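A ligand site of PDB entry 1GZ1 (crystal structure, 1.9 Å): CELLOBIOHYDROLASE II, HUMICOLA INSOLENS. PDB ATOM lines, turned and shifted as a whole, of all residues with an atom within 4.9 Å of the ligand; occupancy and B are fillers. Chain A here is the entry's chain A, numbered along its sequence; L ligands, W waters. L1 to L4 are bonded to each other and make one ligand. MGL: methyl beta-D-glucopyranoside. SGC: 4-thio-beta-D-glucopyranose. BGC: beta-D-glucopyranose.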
ATOM      1  N   TRP A  49     -21.126  22.338   9.587  1.00  0.00           N
ATOM      2  CA  TRP A  49     -21.507  21.049   9.027  1.00  0.00           C
ATOM      3  C   TRP A  49     -21.266  19.862   9.934  1.00  0.00           C
ATOM      4  O   TRP A  49     -20.180  19.777  10.505  1.00  0.00           O
ATOM      5  CB  TRP A  49     -20.706  20.838   7.735  1.00  0.00           C
ATOM      6  CG  TRP A  49     -21.080  21.764   6.634  1.00  0.00           C
ATOM      7  CD1 TRP A  49     -21.083  23.118   6.661  1.00  0.00           C
ATOM      8  CD2 TRP A  49     -21.527  21.392   5.338  1.00  0.00           C
ATOM      9  NE1 TRP A  49     -21.458  23.613   5.430  1.00  0.00           N
ATOM     10  CE2 TRP A  49     -21.751  22.564   4.605  1.00  0.00           C
ATOM     11  CE3 TRP A  49     -21.717  20.162   4.703  1.00  0.00           C
ATOM     12  CZ2 TRP A  49     -22.185  22.547   3.271  1.00  0.00           C
ATOM     13  CZ3 TRP A  49     -22.150  20.121   3.408  1.00  0.00           C
ATOM     14  CH2 TRP A  49     -22.333  21.314   2.675  1.00  0.00           C
ATOM     15  N   ASP A  51     -20.599  16.706   9.160  1.00  0.00           N
ATOM     16  CA  ASP A  51     -20.212  15.900   8.010  1.00  0.00           C
ATOM     17  C   ASP A  51     -19.654  14.527   8.413  1.00  0.00           C
ATOM     18  O   ASP A  51     -19.328  13.695   7.567  1.00  0.00           O
ATOM     19  CB  ASP A  51     -19.170  16.643   7.180  1.00  0.00           C
ATOM     20  CG  ASP A  51     -17.859  16.850   7.930  1.00  0.00           C
ATOM     21  OD1 ASP A  51     -17.889  17.145   9.137  1.00  0.00           O
ATOM     22  OD2 ASP A  51     -16.768  16.734   7.370  1.00  0.00           O
ATOM     23  N   TYR A  86     -25.277  16.131   7.223  1.00  0.00           N
ATOM     24  CA  TYR A  86     -24.551  15.684   6.021  1.00  0.00           C
ATOM     25  C   TYR A  86     -23.811  14.381   6.226  1.00  0.00           C
ATOM     26  O   TYR A  86     -22.570  14.356   6.305  1.00  0.00           O
ATOM     27  CB  TYR A  86     -23.573  16.762   5.615  1.00  0.00           C
ATOM     28  CG  TYR A  86     -22.888  16.519   4.292  1.00  0.00           C
ATOM     29  CD1 TYR A  86     -23.626  16.235   3.142  1.00  0.00           C
ATOM     30  CD2 TYR A  86     -21.506  16.569   4.188  1.00  0.00           C
ATOM     31  CE1 TYR A  86     -22.991  16.008   1.914  1.00  0.00           C
ATOM     32  CE2 TYR A  86     -20.871  16.354   2.972  1.00  0.00           C
ATOM     33  CZ  TYR A  86     -21.594  16.061   1.838  1.00  0.00           C
ATOM     34  OH  TYR A  86     -20.902  15.843   0.634  1.00  0.00           O
ATOM     35  N   ARG A  91     -23.019   8.359   0.547  1.00  0.00           N
ATOM     36  CA  ARG A  91     -23.013   9.789   0.306  1.00  0.00           C
ATOM     37  C   ARG A  91     -22.384  10.181  -1.014  1.00  0.00           C
ATOM     38  O   ARG A  91     -21.408   9.581  -1.439  1.00  0.00           O
ATOM     39  CB  ARG A  91     -22.268  10.518   1.436  1.00  0.00           C
ATOM     40  CG  ARG A  91     -22.847  11.872   1.753  1.00  0.00           C
ATOM     41  CD  ARG A  91     -22.178  12.630   2.903  1.00  0.00           C
ATOM     42  NE  ARG A  91     -20.804  12.989   2.589  1.00  0.00           N
ATOM     43  CZ  ARG A  91     -19.909  13.322   3.491  1.00  0.00           C
ATOM     44  NH1 ARG A  91     -20.242  13.331   4.772  1.00  0.00           N
ATOM     45  NH2 ARG A  91     -18.687  13.661   3.107  1.00  0.00           N
ATOM     46  N   ASP A  92     -22.952  11.195  -1.649  1.00  0.00           N
ATOM     47  CA  ASP A  92     -22.386  11.746  -2.866  1.00  0.00           C
ATOM     48  C   ASP A  92     -22.265  10.643  -3.904  1.00  0.00           C
ATOM     49  O   ASP A  92     -21.174  10.324  -4.404  1.00  0.00           O
ATOM     50  CB  ASP A  92     -21.041  12.392  -2.552  1.00  0.00           C
ATOM     51  CG  ASP A  92     -21.087  13.284  -1.308  1.00  0.00           C
ATOM     52  OD1 ASP A  92     -21.788  14.365  -1.287  1.00  0.00           O
ATOM     53  OD2 ASP A  92     -20.434  12.962  -0.312  1.00  0.00           O
ATOM     54  N   ASN A  99     -16.148  11.039   0.416  1.00  0.00           N
ATOM     55  CA  ASN A  99     -15.625  11.153   1.737  1.00  0.00           C
ATOM     56  C   ASN A  99     -16.627  10.675   2.782  1.00  0.00           C
ATOM     57  O   ASN A  99     -16.280  10.573   3.942  1.00  0.00           O
ATOM     58  CB  ASN A  99     -15.208  12.587   2.064  1.00  0.00           C
ATOM     59  CG  ASN A  99     -14.338  13.190   0.968  1.00  0.00           C
ATOM     60  OD1 ASN A  99     -13.136  13.355   1.149  1.00  0.00           O
ATOM     61  ND2 ASN A  99     -14.972  13.527  -0.182  1.00  0.00           N
ATOM     62  N   PRO A 137     -27.039  18.194   1.687  1.00  0.00           N
ATOM     63  CA  PRO A 137     -26.575  18.653   0.392  1.00  0.00           C
ATOM     64  C   PRO A 137     -26.092  17.505  -0.478  1.00  0.00           C
ATOM     65  O   PRO A 137     -25.608  16.457   0.030  1.00  0.00           O
ATOM     66  CB  PRO A 137     -25.400  19.578   0.759  1.00  0.00           C
ATOM     67  CG  PRO A 137     -25.802  20.135   2.063  1.00  0.00           C
ATOM     68  CD  PRO A 137     -26.408  18.928   2.792  1.00  0.00           C
ATOM     69  N   ASP A 138     -26.243  17.683  -1.786  1.00  0.00           N
ATOM     70  CA  ASP A 138     -25.708  16.735  -2.766  1.00  0.00           C
ATOM     71  C   ASP A 138     -26.339  15.365  -2.635  1.00  0.00           C
ATOM     72  O   ASP A 138     -25.665  14.369  -2.761  1.00  0.00           O
ATOM     73  CB  ASP A 138     -24.164  16.625  -2.643  1.00  0.00           C
ATOM     74  CG  ASP A 138     -23.543  15.886  -3.818  1.00  0.00           C
ATOM     75  OD1 ASP A 138     -24.124  16.007  -4.917  1.00  0.00           O
ATOM     76  OD2 ASP A 138     -22.513  15.167  -3.747  1.00  0.00           O
ATOM     77  N   ASN A 142     -29.360  14.405  -7.094  1.00  0.00           N
ATOM     78  CA  ASN A 142     -28.819  13.374  -7.962  1.00  0.00           C
ATOM     79  C   ASN A 142     -29.903  12.473  -8.538  1.00  0.00           C
ATOM     80  O   ASN A 142     -29.719  11.849  -9.587  1.00  0.00           O
ATOM     81  CB  ASN A 142     -27.783  12.543  -7.196  1.00  0.00           C
ATOM     82  CG  ASN A 142     -26.534  13.326  -6.933  1.00  0.00           C
ATOM     83  OD1 ASN A 142     -25.811  13.650  -7.858  1.00  0.00           O
ATOM     84  ND2 ASN A 142     -26.319  13.710  -5.675  1.00  0.00           N
ATOM     85  N   THR A 145     -31.091  13.906 -11.949  1.00  0.00           N
ATOM     86  CA  THR A 145     -30.256  13.859 -13.138  1.00  0.00           C
ATOM     87  C   THR A 145     -29.304  12.710 -13.224  1.00  0.00           C
ATOM     88  O   THR A 145     -28.814  12.482 -14.307  1.00  0.00           O
ATOM     89  CB  THR A 145     -29.411  15.142 -13.271  1.00  0.00           C
ATOM     90  OG1 THR A 145     -28.534  15.268 -12.142  1.00  0.00           O
ATOM     91  CG2 THR A 145     -30.262  16.363 -13.249  1.00  0.00           C
ATOM     92  N   ASN A 146     -29.021  11.990 -12.152  1.00  0.00           N
ATOM     93  CA  ASN A 146     -27.977  10.964 -12.173  1.00  0.00           C
ATOM     94  C   ASN A 146     -28.446   9.521 -12.003  1.00  0.00           C
ATOM     95  O   ASN A 146     -27.673   8.669 -11.601  1.00  0.00           O
ATOM     96  CB  ASN A 146     -26.908  11.329 -11.141  1.00  0.00           C
ATOM     97  CG  ASN A 146     -26.033  12.475 -11.619  1.00  0.00           C
ATOM     98  OD1 ASN A 146     -25.705  12.547 -12.808  1.00  0.00           O
ATOM     99  ND2 ASN A 146     -25.637  13.348 -10.699  1.00  0.00           N
ATOM    100  N   HIS A 183     -29.095  23.630  -7.679  1.00  0.00           N
ATOM    101  CA  HIS A 183     -28.984  25.017  -8.049  1.00  0.00           C
ATOM    102  C   HIS A 183     -29.447  25.258  -9.476  1.00  0.00           C
ATOM    103  O   HIS A 183     -29.765  24.317 -10.210  1.00  0.00           O
ATOM    104  CB  HIS A 183     -27.534  25.508  -7.894  1.00  0.00           C
ATOM    105  CG  HIS A 183     -26.573  24.807  -8.792  1.00  0.00           C
ATOM    106  ND1 HIS A 183     -26.337  25.204 -10.085  1.00  0.00           N
ATOM    107  CD2 HIS A 183     -25.749  23.752  -8.561  1.00  0.00           C
ATOM    108  CE1 HIS A 183     -25.451  24.392 -10.635  1.00  0.00           C
ATOM    109  NE2 HIS A 183     -25.086  23.496  -9.740  1.00  0.00           N
ATOM    110  N   GLY A 185     -28.138  25.746 -12.196  1.00  0.00           N
ATOM    111  CA  GLY A 185     -27.449  25.041 -13.249  1.00  0.00           C
ATOM    112  C   GLY A 185     -27.554  23.536 -13.191  1.00  0.00           C
ATOM    113  O   GLY A 185     -27.001  22.840 -14.015  1.00  0.00           O
ATOM    114  N   TRP A 186     -28.259  23.044 -12.195  1.00  0.00           N
ATOM    115  CA  TRP A 186     -28.406  21.624 -11.991  1.00  0.00           C
ATOM    116  C   TRP A 186     -29.865  21.266 -12.258  1.00  0.00           C
ATOM    117  O   TRP A 186     -30.161  20.578 -13.221  1.00  0.00           O
ATOM    118  CB  TRP A 186     -28.046  21.273 -10.559  1.00  0.00           C
ATOM    119  CG  TRP A 186     -27.903  19.812 -10.320  1.00  0.00           C
ATOM    120  CD1 TRP A 186     -28.308  18.795 -11.123  1.00  0.00           C
ATOM    121  CD2 TRP A 186     -27.319  19.193  -9.182  1.00  0.00           C
ATOM    122  NE1 TRP A 186     -27.994  17.587 -10.565  1.00  0.00           N
ATOM    123  CE2 TRP A 186     -27.379  17.813  -9.363  1.00  0.00           C
ATOM    124  CE3 TRP A 186     -26.718  19.695  -8.011  1.00  0.00           C
ATOM    125  CZ2 TRP A 186     -26.875  16.921  -8.428  1.00  0.00           C
ATOM    126  CZ3 TRP A 186     -26.220  18.806  -7.095  1.00  0.00           C
ATOM    127  CH2 TRP A 186     -26.324  17.431  -7.293  1.00  0.00           C
ATOM    128  N   VAL A 220     -26.071  25.571  -2.630  1.00  0.00           N
ATOM    129  CA  VAL A 220     -25.185  25.115  -1.575  1.00  0.00           C
ATOM    130  C   VAL A 220     -23.894  24.615  -2.185  1.00  0.00           C
ATOM    131  O   VAL A 220     -23.890  23.715  -2.999  1.00  0.00           O
ATOM    132  CB  VAL A 220     -25.843  23.995  -0.782  1.00  0.00           C
ATOM    133  CG1 VAL A 220     -24.908  23.505   0.261  1.00  0.00           C
ATOM    134  CG2 VAL A 220     -27.127  24.480  -0.134  1.00  0.00           C
ATOM    135  N   ALA A 221     -22.790  25.203  -1.736  1.00  0.00           N
ATOM    136  CA  ALA A 221     -21.462  24.892  -2.218  1.00  0.00           C
ATOM    137  C   ALA A 221     -21.236  25.239  -3.656  1.00  0.00           C
ATOM    138  O   ALA A 221     -20.231  24.844  -4.194  1.00  0.00           O
ATOM    139  CB  ALA A 221     -21.069  23.468  -1.950  1.00  0.00           C
ATOM    140  N   ASN A 222     -22.146  25.980  -4.267  1.00  0.00           N
ATOM    141  CA  ASN A 222     -21.933  26.402  -5.622  1.00  0.00           C
ATOM    142  C   ASN A 222     -21.675  27.924  -5.686  1.00  0.00           C
ATOM    143  O   ASN A 222     -21.494  28.588  -4.623  1.00  0.00           O
ATOM    144  CB  ASN A 222     -23.058  25.899  -6.531  1.00  0.00           C
ATOM    145  CG  ASN A 222     -22.574  25.607  -7.955  1.00  0.00           C
ATOM    146  OD1 ASN A 222     -22.416  26.512  -8.757  1.00  0.00           O
ATOM    147  ND2 ASN A 222     -22.274  24.338  -8.238  1.00  0.00           N
ATOM    148  N   ARG A 269     -19.846  32.038  -1.979  1.00  0.00           N
ATOM    149  CA  ARG A 269     -18.804  32.150  -2.995  1.00  0.00           C
ATOM    150  C   ARG A 269     -19.369  32.710  -4.311  1.00  0.00           C
ATOM    151  O   ARG A 269     -18.910  32.333  -5.377  1.00  0.00           O
ATOM    152  CB  ARG A 269     -18.132  30.797  -3.226  1.00  0.00           C
ATOM    153  CG  ARG A 269     -17.611  30.143  -1.944  1.00  0.00           C
ATOM    154  CD  ARG A 269     -16.655  28.948  -2.147  1.00  0.00           C
ATOM    155  NE  ARG A 269     -17.411  27.781  -2.569  1.00  0.00           N
ATOM    156  CZ  ARG A 269     -16.888  26.621  -2.909  1.00  0.00           C
ATOM    157  NH1 ARG A 269     -15.564  26.416  -2.856  1.00  0.00           N
ATOM    158  NH2 ARG A 269     -17.685  25.642  -3.284  1.00  0.00           N
ATOM    159  N   TRP A 280     -20.484  25.388 -16.767  1.00  0.00           N
ATOM    160  CA  TRP A 280     -21.277  25.542 -15.542  1.00  0.00           C
ATOM    161  C   TRP A 280     -21.178  24.384 -14.560  1.00  0.00           C
ATOM    162  O   TRP A 280     -21.303  24.586 -13.358  1.00  0.00           O
ATOM    163  CB  TRP A 280     -22.733  25.761 -15.900  1.00  0.00           C
ATOM    164  CG  TRP A 280     -23.540  26.588 -14.978  1.00  0.00           C
ATOM    165  CD1 TRP A 280     -23.161  27.135 -13.789  1.00  0.00           C
ATOM    166  CD2 TRP A 280     -24.905  26.960 -15.179  1.00  0.00           C
ATOM    167  NE1 TRP A 280     -24.204  27.814 -13.231  1.00  0.00           N
ATOM    168  CE2 TRP A 280     -25.288  27.725 -14.069  1.00  0.00           C
ATOM    169  CE3 TRP A 280     -25.834  26.730 -16.202  1.00  0.00           C
ATOM    170  CZ2 TRP A 280     -26.563  28.272 -13.949  1.00  0.00           C
ATOM    171  CZ3 TRP A 280     -27.098  27.270 -16.076  1.00  0.00           C
ATOM    172  CH2 TRP A 280     -27.454  28.028 -14.954  1.00  0.00           C
ATOM    173  N   GLY A 281     -20.972  23.167 -15.070  1.00  0.00           N
ATOM    174  CA  GLY A 281     -20.920  21.985 -14.238  1.00  0.00           C
ATOM    175  C   GLY A 281     -19.605  21.773 -13.542  1.00  0.00           C
ATOM    176  O   GLY A 281     -19.387  20.772 -12.861  1.00  0.00           O
ATOM    177  N   TRP A 283     -17.787  22.279 -10.748  1.00  0.00           N
ATOM    178  CA  TRP A 283     -18.103  22.587  -9.356  1.00  0.00           C
ATOM    179  C   TRP A 283     -16.980  22.636  -8.314  1.00  0.00           C
ATOM    180  O   TRP A 283     -17.220  23.107  -7.207  1.00  0.00           O
ATOM    181  CB  TRP A 283     -19.115  21.550  -8.856  1.00  0.00           C
ATOM    182  CG  TRP A 283     -18.637  20.133  -8.926  1.00  0.00           C
ATOM    183  CD1 TRP A 283     -18.846  19.235  -9.945  1.00  0.00           C
ATOM    184  CD2 TRP A 283     -17.862  19.445  -7.950  1.00  0.00           C
ATOM    185  NE1 TRP A 283     -18.242  18.031  -9.645  1.00  0.00           N
ATOM    186  CE2 TRP A 283     -17.615  18.140  -8.436  1.00  0.00           C
ATOM    187  CE3 TRP A 283     -17.325  19.800  -6.720  1.00  0.00           C
ATOM    188  CZ2 TRP A 283     -16.902  17.190  -7.699  1.00  0.00           C
ATOM    189  CZ3 TRP A 283     -16.605  18.880  -6.013  1.00  0.00           C
ATOM    190  CH2 TRP A 283     -16.390  17.585  -6.497  1.00  0.00           C
ATOM    191  N   LYS A 311     -21.819  26.760   2.428  1.00  0.00           N
ATOM    192  CA  LYS A 311     -20.502  26.194   2.258  1.00  0.00           C
ATOM    193  C   LYS A 311     -19.541  27.241   2.826  1.00  0.00           C
ATOM    194  O   LYS A 311     -19.621  28.392   2.404  1.00  0.00           O
ATOM    195  CB  LYS A 311     -20.266  25.937   0.785  1.00  0.00           C
ATOM    196  CG  LYS A 311     -18.816  25.632   0.413  1.00  0.00           C
ATOM    197  CD  LYS A 311     -18.320  24.350   1.024  1.00  0.00           C
ATOM    198  CE  LYS A 311     -16.844  24.117   0.710  1.00  0.00           C
ATOM    199  NZ  LYS A 311     -16.353  22.751   1.073  1.00  0.00           N
ATOM    200  N   PRO A 312     -18.691  26.915   3.798  1.00  0.00           N
ATOM    201  CA  PRO A 312     -17.775  27.929   4.321  1.00  0.00           C
ATOM    202  C   PRO A 312     -16.571  28.144   3.439  1.00  0.00           C
ATOM    203  O   PRO A 312     -15.730  27.288   3.314  1.00  0.00           O
ATOM    204  CB  PRO A 312     -17.378  27.367   5.704  1.00  0.00           C
ATOM    205  CG  PRO A 312     -18.447  26.284   5.979  1.00  0.00           C
ATOM    206  CD  PRO A 312     -18.587  25.683   4.593  1.00  0.00           C
ATOM    207  N   GLU A 315     -12.881  26.245   2.875  1.00  0.00           N
ATOM    208  CA  GLU A 315     -12.912  24.807   3.102  1.00  0.00           C
ATOM    209  C   GLU A 315     -13.013  24.130   1.721  1.00  0.00           C
ATOM    210  O   GLU A 315     -13.903  24.422   0.939  1.00  0.00           O
ATOM    211  CB  GLU A 315     -14.052  24.393   4.033  1.00  0.00           C
ATOM    212  CG  GLU A 315     -13.829  24.831   5.480  1.00  0.00           C
ATOM    213  CD  GLU A 315     -15.002  24.524   6.400  1.00  0.00           C
ATOM    214  OE1 GLU A 315     -15.952  23.736   6.024  1.00  0.00           O
ATOM    215  OE2 GLU A 315     -14.950  25.038   7.533  1.00  0.00           O
ATOM    216  N   CYS A 316     -12.092  23.211   1.440  1.00  0.00           N
ATOM    217  CA  CYS A 316     -11.916  22.639   0.124  1.00  0.00           C
ATOM    218  C   CYS A 316     -13.126  21.852  -0.389  1.00  0.00           C
ATOM    219  O   CYS A 316     -13.873  21.292   0.395  1.00  0.00           O
ATOM    220  CB  CYS A 316     -10.734  21.666   0.152  1.00  0.00           C
ATOM    221  SG  CYS A 316     -10.045  21.294  -1.473  1.00  0.00           S
ATOM    222  N   ASP A 317     -13.247  21.741  -1.695  1.00  0.00           N
ATOM    223  CA  ASP A 317     -14.358  20.944  -2.264  1.00  0.00           C
ATOM    224  C   ASP A 317     -13.929  19.523  -2.574  1.00  0.00           C
ATOM    225  O   ASP A 317     -14.776  18.626  -2.758  1.00  0.00           O
ATOM    226  CB  ASP A 317     -14.847  21.562  -3.562  1.00  0.00           C
ATOM    227  CG  ASP A 317     -15.393  22.922  -3.383  1.00  0.00           C
ATOM    228  OD1 ASP A 317     -16.149  23.158  -2.402  1.00  0.00           O
ATOM    229  OD2 ASP A 317     -15.094  23.852  -4.175  1.00  0.00           O
ATOM    230  N   ALA A 343     -11.444  17.135   0.659  1.00  0.00           N
ATOM    231  CA  ALA A 343     -12.677  17.876   0.853  1.00  0.00           C
ATOM    232  C   ALA A 343     -12.883  18.187   2.336  1.00  0.00           C
ATOM    233  O   ALA A 343     -12.739  17.319   3.193  1.00  0.00           O
ATOM    234  CB  ALA A 343     -13.843  17.070   0.322  1.00  0.00           C
ATOM    235  N   GLY A 344     -13.223  19.434   2.597  1.00  0.00           N
ATOM    236  CA  GLY A 344     -13.531  19.903   3.929  1.00  0.00           C
ATOM    237  C   GLY A 344     -12.323  20.458   4.626  1.00  0.00           C
ATOM    238  O   GLY A 344     -12.432  21.113   5.646  1.00  0.00           O
HETATM  239  C1  MGL L   1     -24.536  19.594 -12.671  1.00  0.00           C
HETATM  240  C2  MGL L   1     -24.341  20.674 -11.625  1.00  0.00           C
HETATM  241  C3  MGL L   1     -23.205  20.305 -10.704  1.00  0.00           C
HETATM  242  C4  MGL L   1     -23.393  18.882 -10.186  1.00  0.00           C
HETATM  243  C5  MGL L   1     -23.620  17.917 -11.340  1.00  0.00           C
HETATM  244  C6  MGL L   1     -23.824  16.516 -10.835  1.00  0.00           C
HETATM  245  C7  MGL L   1     -26.184  18.846 -14.217  1.00  0.00           C
HETATM  246  O1  MGL L   1     -25.669  19.943 -13.469  1.00  0.00           O
HETATM  247  O2  MGL L   1     -24.018  21.886 -12.290  1.00  0.00           O
HETATM  248  O3  MGL L   1     -23.118  21.253  -9.656  1.00  0.00           O
HETATM  249  O4  MGL L   1     -22.230  18.460  -9.466  1.00  0.00           O
HETATM  250  O5  MGL L   1     -24.773  18.358 -12.040  1.00  0.00           O
HETATM  251  O6  MGL L   1     -23.968  15.571 -11.895  1.00  0.00           O
HETATM  252  C1  SGC L   2     -22.307  18.279  -7.995  1.00  0.00           C
HETATM  253  C2  SGC L   2     -21.035  17.584  -7.552  1.00  0.00           C
HETATM  254  O2  SGC L   2     -21.058  16.225  -7.967  1.00  0.00           O
HETATM  255  C3  SGC L   2     -20.866  17.636  -6.048  1.00  0.00           C
HETATM  256  O3  SGC L   2     -19.642  17.134  -5.555  1.00  0.00           O
HETATM  257  C4  SGC L   2     -21.033  19.156  -5.498  1.00  0.00           C
HETATM  258  C5  SGC L   2     -22.218  19.900  -6.197  1.00  0.00           C
HETATM  259  O5  SGC L   2     -22.318  19.671  -7.616  1.00  0.00           O
HETATM  260  C6  SGC L   2     -22.046  21.408  -6.030  1.00  0.00           C
HETATM  261  O6  SGC L   2     -23.148  22.057  -6.517  1.00  0.00           O
HETATM  262  S4  SGC L   2     -21.354  19.319  -3.723  1.00  0.00           S
HETATM  263  C2  BGC L   3     -19.106  20.431  -2.636  1.00  0.00           C
HETATM  264  C3  BGC L   3     -18.168  20.251  -1.444  1.00  0.00           C
HETATM  265  C4  BGC L   3     -18.900  19.706  -0.223  1.00  0.00           C
HETATM  266  C5  BGC L   3     -19.912  18.618  -0.610  1.00  0.00           C
HETATM  267  C6  BGC L   3     -21.376  19.006  -0.454  1.00  0.00           C
HETATM  268  C1  BGC L   3     -19.701  19.082  -2.996  1.00  0.00           C
HETATM  269  O2  BGC L   3     -18.379  21.037  -3.705  1.00  0.00           O
HETATM  270  O3  BGC L   3     -17.655  21.508  -1.116  1.00  0.00           O
HETATM  271  O4  BGC L   3     -17.847  19.129   0.528  1.00  0.00           O
HETATM  272  O5  BGC L   3     -19.591  18.166  -1.911  1.00  0.00           O
HETATM  273  O6  BGC L   3     -21.551  20.332  -0.866  1.00  0.00           O
HETATM  274  C2  BGC L   4     -17.026  18.269   2.689  1.00  0.00           C
HETATM  275  C3  BGC L   4     -17.275  18.306   4.192  1.00  0.00           C
HETATM  276  C4  BGC L   4     -17.354  19.728   4.717  1.00  0.00           C
HETATM  277  C5  BGC L   4     -18.308  20.559   3.870  1.00  0.00           C
HETATM  278  C6  BGC L   4     -18.301  22.034   4.214  1.00  0.00           C
HETATM  279  C1  BGC L   4     -17.878  19.329   1.966  1.00  0.00           C
HETATM  280  O2  BGC L   4     -17.221  16.945   2.274  1.00  0.00           O
HETATM  281  O3  BGC L   4     -16.242  17.617   4.845  1.00  0.00           O
HETATM  282  O4  BGC L   4     -17.897  19.714   6.032  1.00  0.00           O
HETATM  283  O5  BGC L   4     -18.046  20.582   2.501  1.00  0.00           O
HETATM  284  O6  BGC L   4     -17.074  22.613   3.839  1.00  0.00           O
HETATM  285  O   HOH W   1     -14.954  15.388   3.299  1.00  0.00           O
HETATM  286  O   HOH W   2     -23.993  20.980  -2.057  1.00  0.00           O
HETATM  287  O   HOH W   3     -14.348  17.987   7.675  1.00  0.00           O
HETATM  288  O   HOH W   4     -20.052  15.797 -10.608  1.00  0.00           O
HETATM  289  O   HOH W   5     -21.508  15.449 -12.639  1.00  0.00           O
HETATM  290  O   HOH W   6     -17.055  14.559   5.380  1.00  0.00           O
HETATM  291  O   HOH W   7     -25.969  15.232 -13.528  1.00  0.00           O
HETATM  292  O   HOH W   8     -16.897  21.742   7.434  1.00  0.00           O
HETATM  293  O   HOH W   9     -25.584  22.820  -4.897  1.00  0.00           O
HETATM  294  O   HOH W  10     -19.200  22.752  -5.372  1.00  0.00           O
HETATM  295  O   HOH W  11     -17.561  15.775  -0.023  1.00  0.00           O
HETATM  296  O   HOH W  12     -21.275  23.395 -10.807  1.00  0.00           O
HETATM  297  O   HOH W  13     -23.458  15.120  -7.353  1.00  0.00           O
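Water W10 lies within hydrogen-bond range of O2 of BGC L3, O of Ala 221 and O of Trp 283. Water W2 bridges an oxygen (O6) of BGC L3 and the backbone carbonyl oxygen (O) of Val 220. Water W4 bridges O2 of SGC L2 (2.9 Å) and NE1 of Trp 283 (3.0 Å). Water W9 bridges the backbone carbonyl oxygen (O) of Val 220 (2.7 Å) and an oxygen (O6) of SGC L2 (3.0 Å). Water W12 lies within hydrogen-bond range of the backbone carbonyl oxygen (O) of Trp 280 (2.8 Å), the side-chain amide nitrogen (ND2) of Asn 222 (2.9 Å) and an oxygen (O3) of MGL L1 (3.1 Å). Water W6 lies within hydrogen-bond range of the guanidinium group of Arg 91, the side-chain carboxylate of Asp 51 and an oxygen (O3) of BGC L4.
O1 of MGL L1 lies close to O of Gly 185 (3.2 Å). CB of Trp 49 touches O4 of BGC L4 (3.5 Å). OH of Tyr 86 touches C5 of BGC L3, 3.2 Å away. NH2 of Arg 91 touches O2 of BGC L4 (3.7 Å). OD2 of Asp 138 touches C3 of SGC L2 (3.8 Å). CA of Trp 186 touches O1 of MGL L1, 3.5 Å away. O of Val 220 touches O6 of SGC L2, at 3.96 Å. CB of Ala 221 touches O6 of BGC L3 (3.4 Å). O of Trp 280 touches O2 of MGL L1, at 3.98 Å. Gly 281 touches the ligand. Trp 283 touches the ligand. Pro 312 touches the ligand. O of Ala 343 touches O3 of BGC L4 (3.9 Å). CA of Gly 344 touches O3 of BGC L4 (3.7 Å). Hydrophobic or aromatic side chains that line the ligand: Trp 49, Tyr 86, His 183, Trp 186, Ala 221, Trp 283, Pro 312 and Ala 343. Of the 28 residues printed, 21 come within 4 Å of the ligand.
OD2 of Asp 92 lies within salt-bridge range of NE of Arg 91, 2.9 Å away. The backbone carbonyl oxygen of Ala 221 sits at hydrogen-bond distance from the guanidinium group of Arg 269 (2.8 Å). The guanidinium group (NH1) of Arg 91 sits at hydrogen-bond distance from the backbone carbonyl oxygen (O) of Asp 51 (3.0 Å). A ring nitrogen (ND1) of His 183 lies within hydrogen-bond range of the backbone NH (N) of Gly 185, at 2.8 Å. The backbone NH (N) of Gly 344 is in hydrogen-bond range of the backbone carbonyl oxygen (O) of Cys 316, 3.0 Å away. NE1 of Trp 186 sits at hydrogen-bond distance from OG1 of Thr 145, 2.9 Å away. O of Glu 315 lies close to NZ of Lys 311, at 3.0 Å. OD1 of Asp 317 is in salt-bridge range of NZ of Lys 311, at 3.5 Å.
An oxygen (O6) of SGC L2 is in hydrogen-bond range of the side-chain amide nitrogen (ND2) of Asn 222 (3.0 Å). An oxygen (O6) of MGL L1 lies within hydrogen-bond range of the side-chain amide nitrogen (ND2) of Asn 146 (3.0 Å). O3 of BGC L3 sits at hydrogen-bond distance from NZ of Lys 311, 2.8 Å away. O6 of BGC L4 is in hydrogen-bond range of OE1 of Glu 315. A ring nitrogen (NE2) of His 183 sits at hydrogen-bond distance from an oxygen (O3) of MGL L1 (3.0 Å). An oxygen (O3) of BGC L4 sits at hydrogen-bond distance from the side-chain carboxylate (OD2) of Asp 51, at 2.7 Å. OD1 of Asp 317 lies within hydrogen-bond range of O3 of BGC L3 (2.6 Å).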
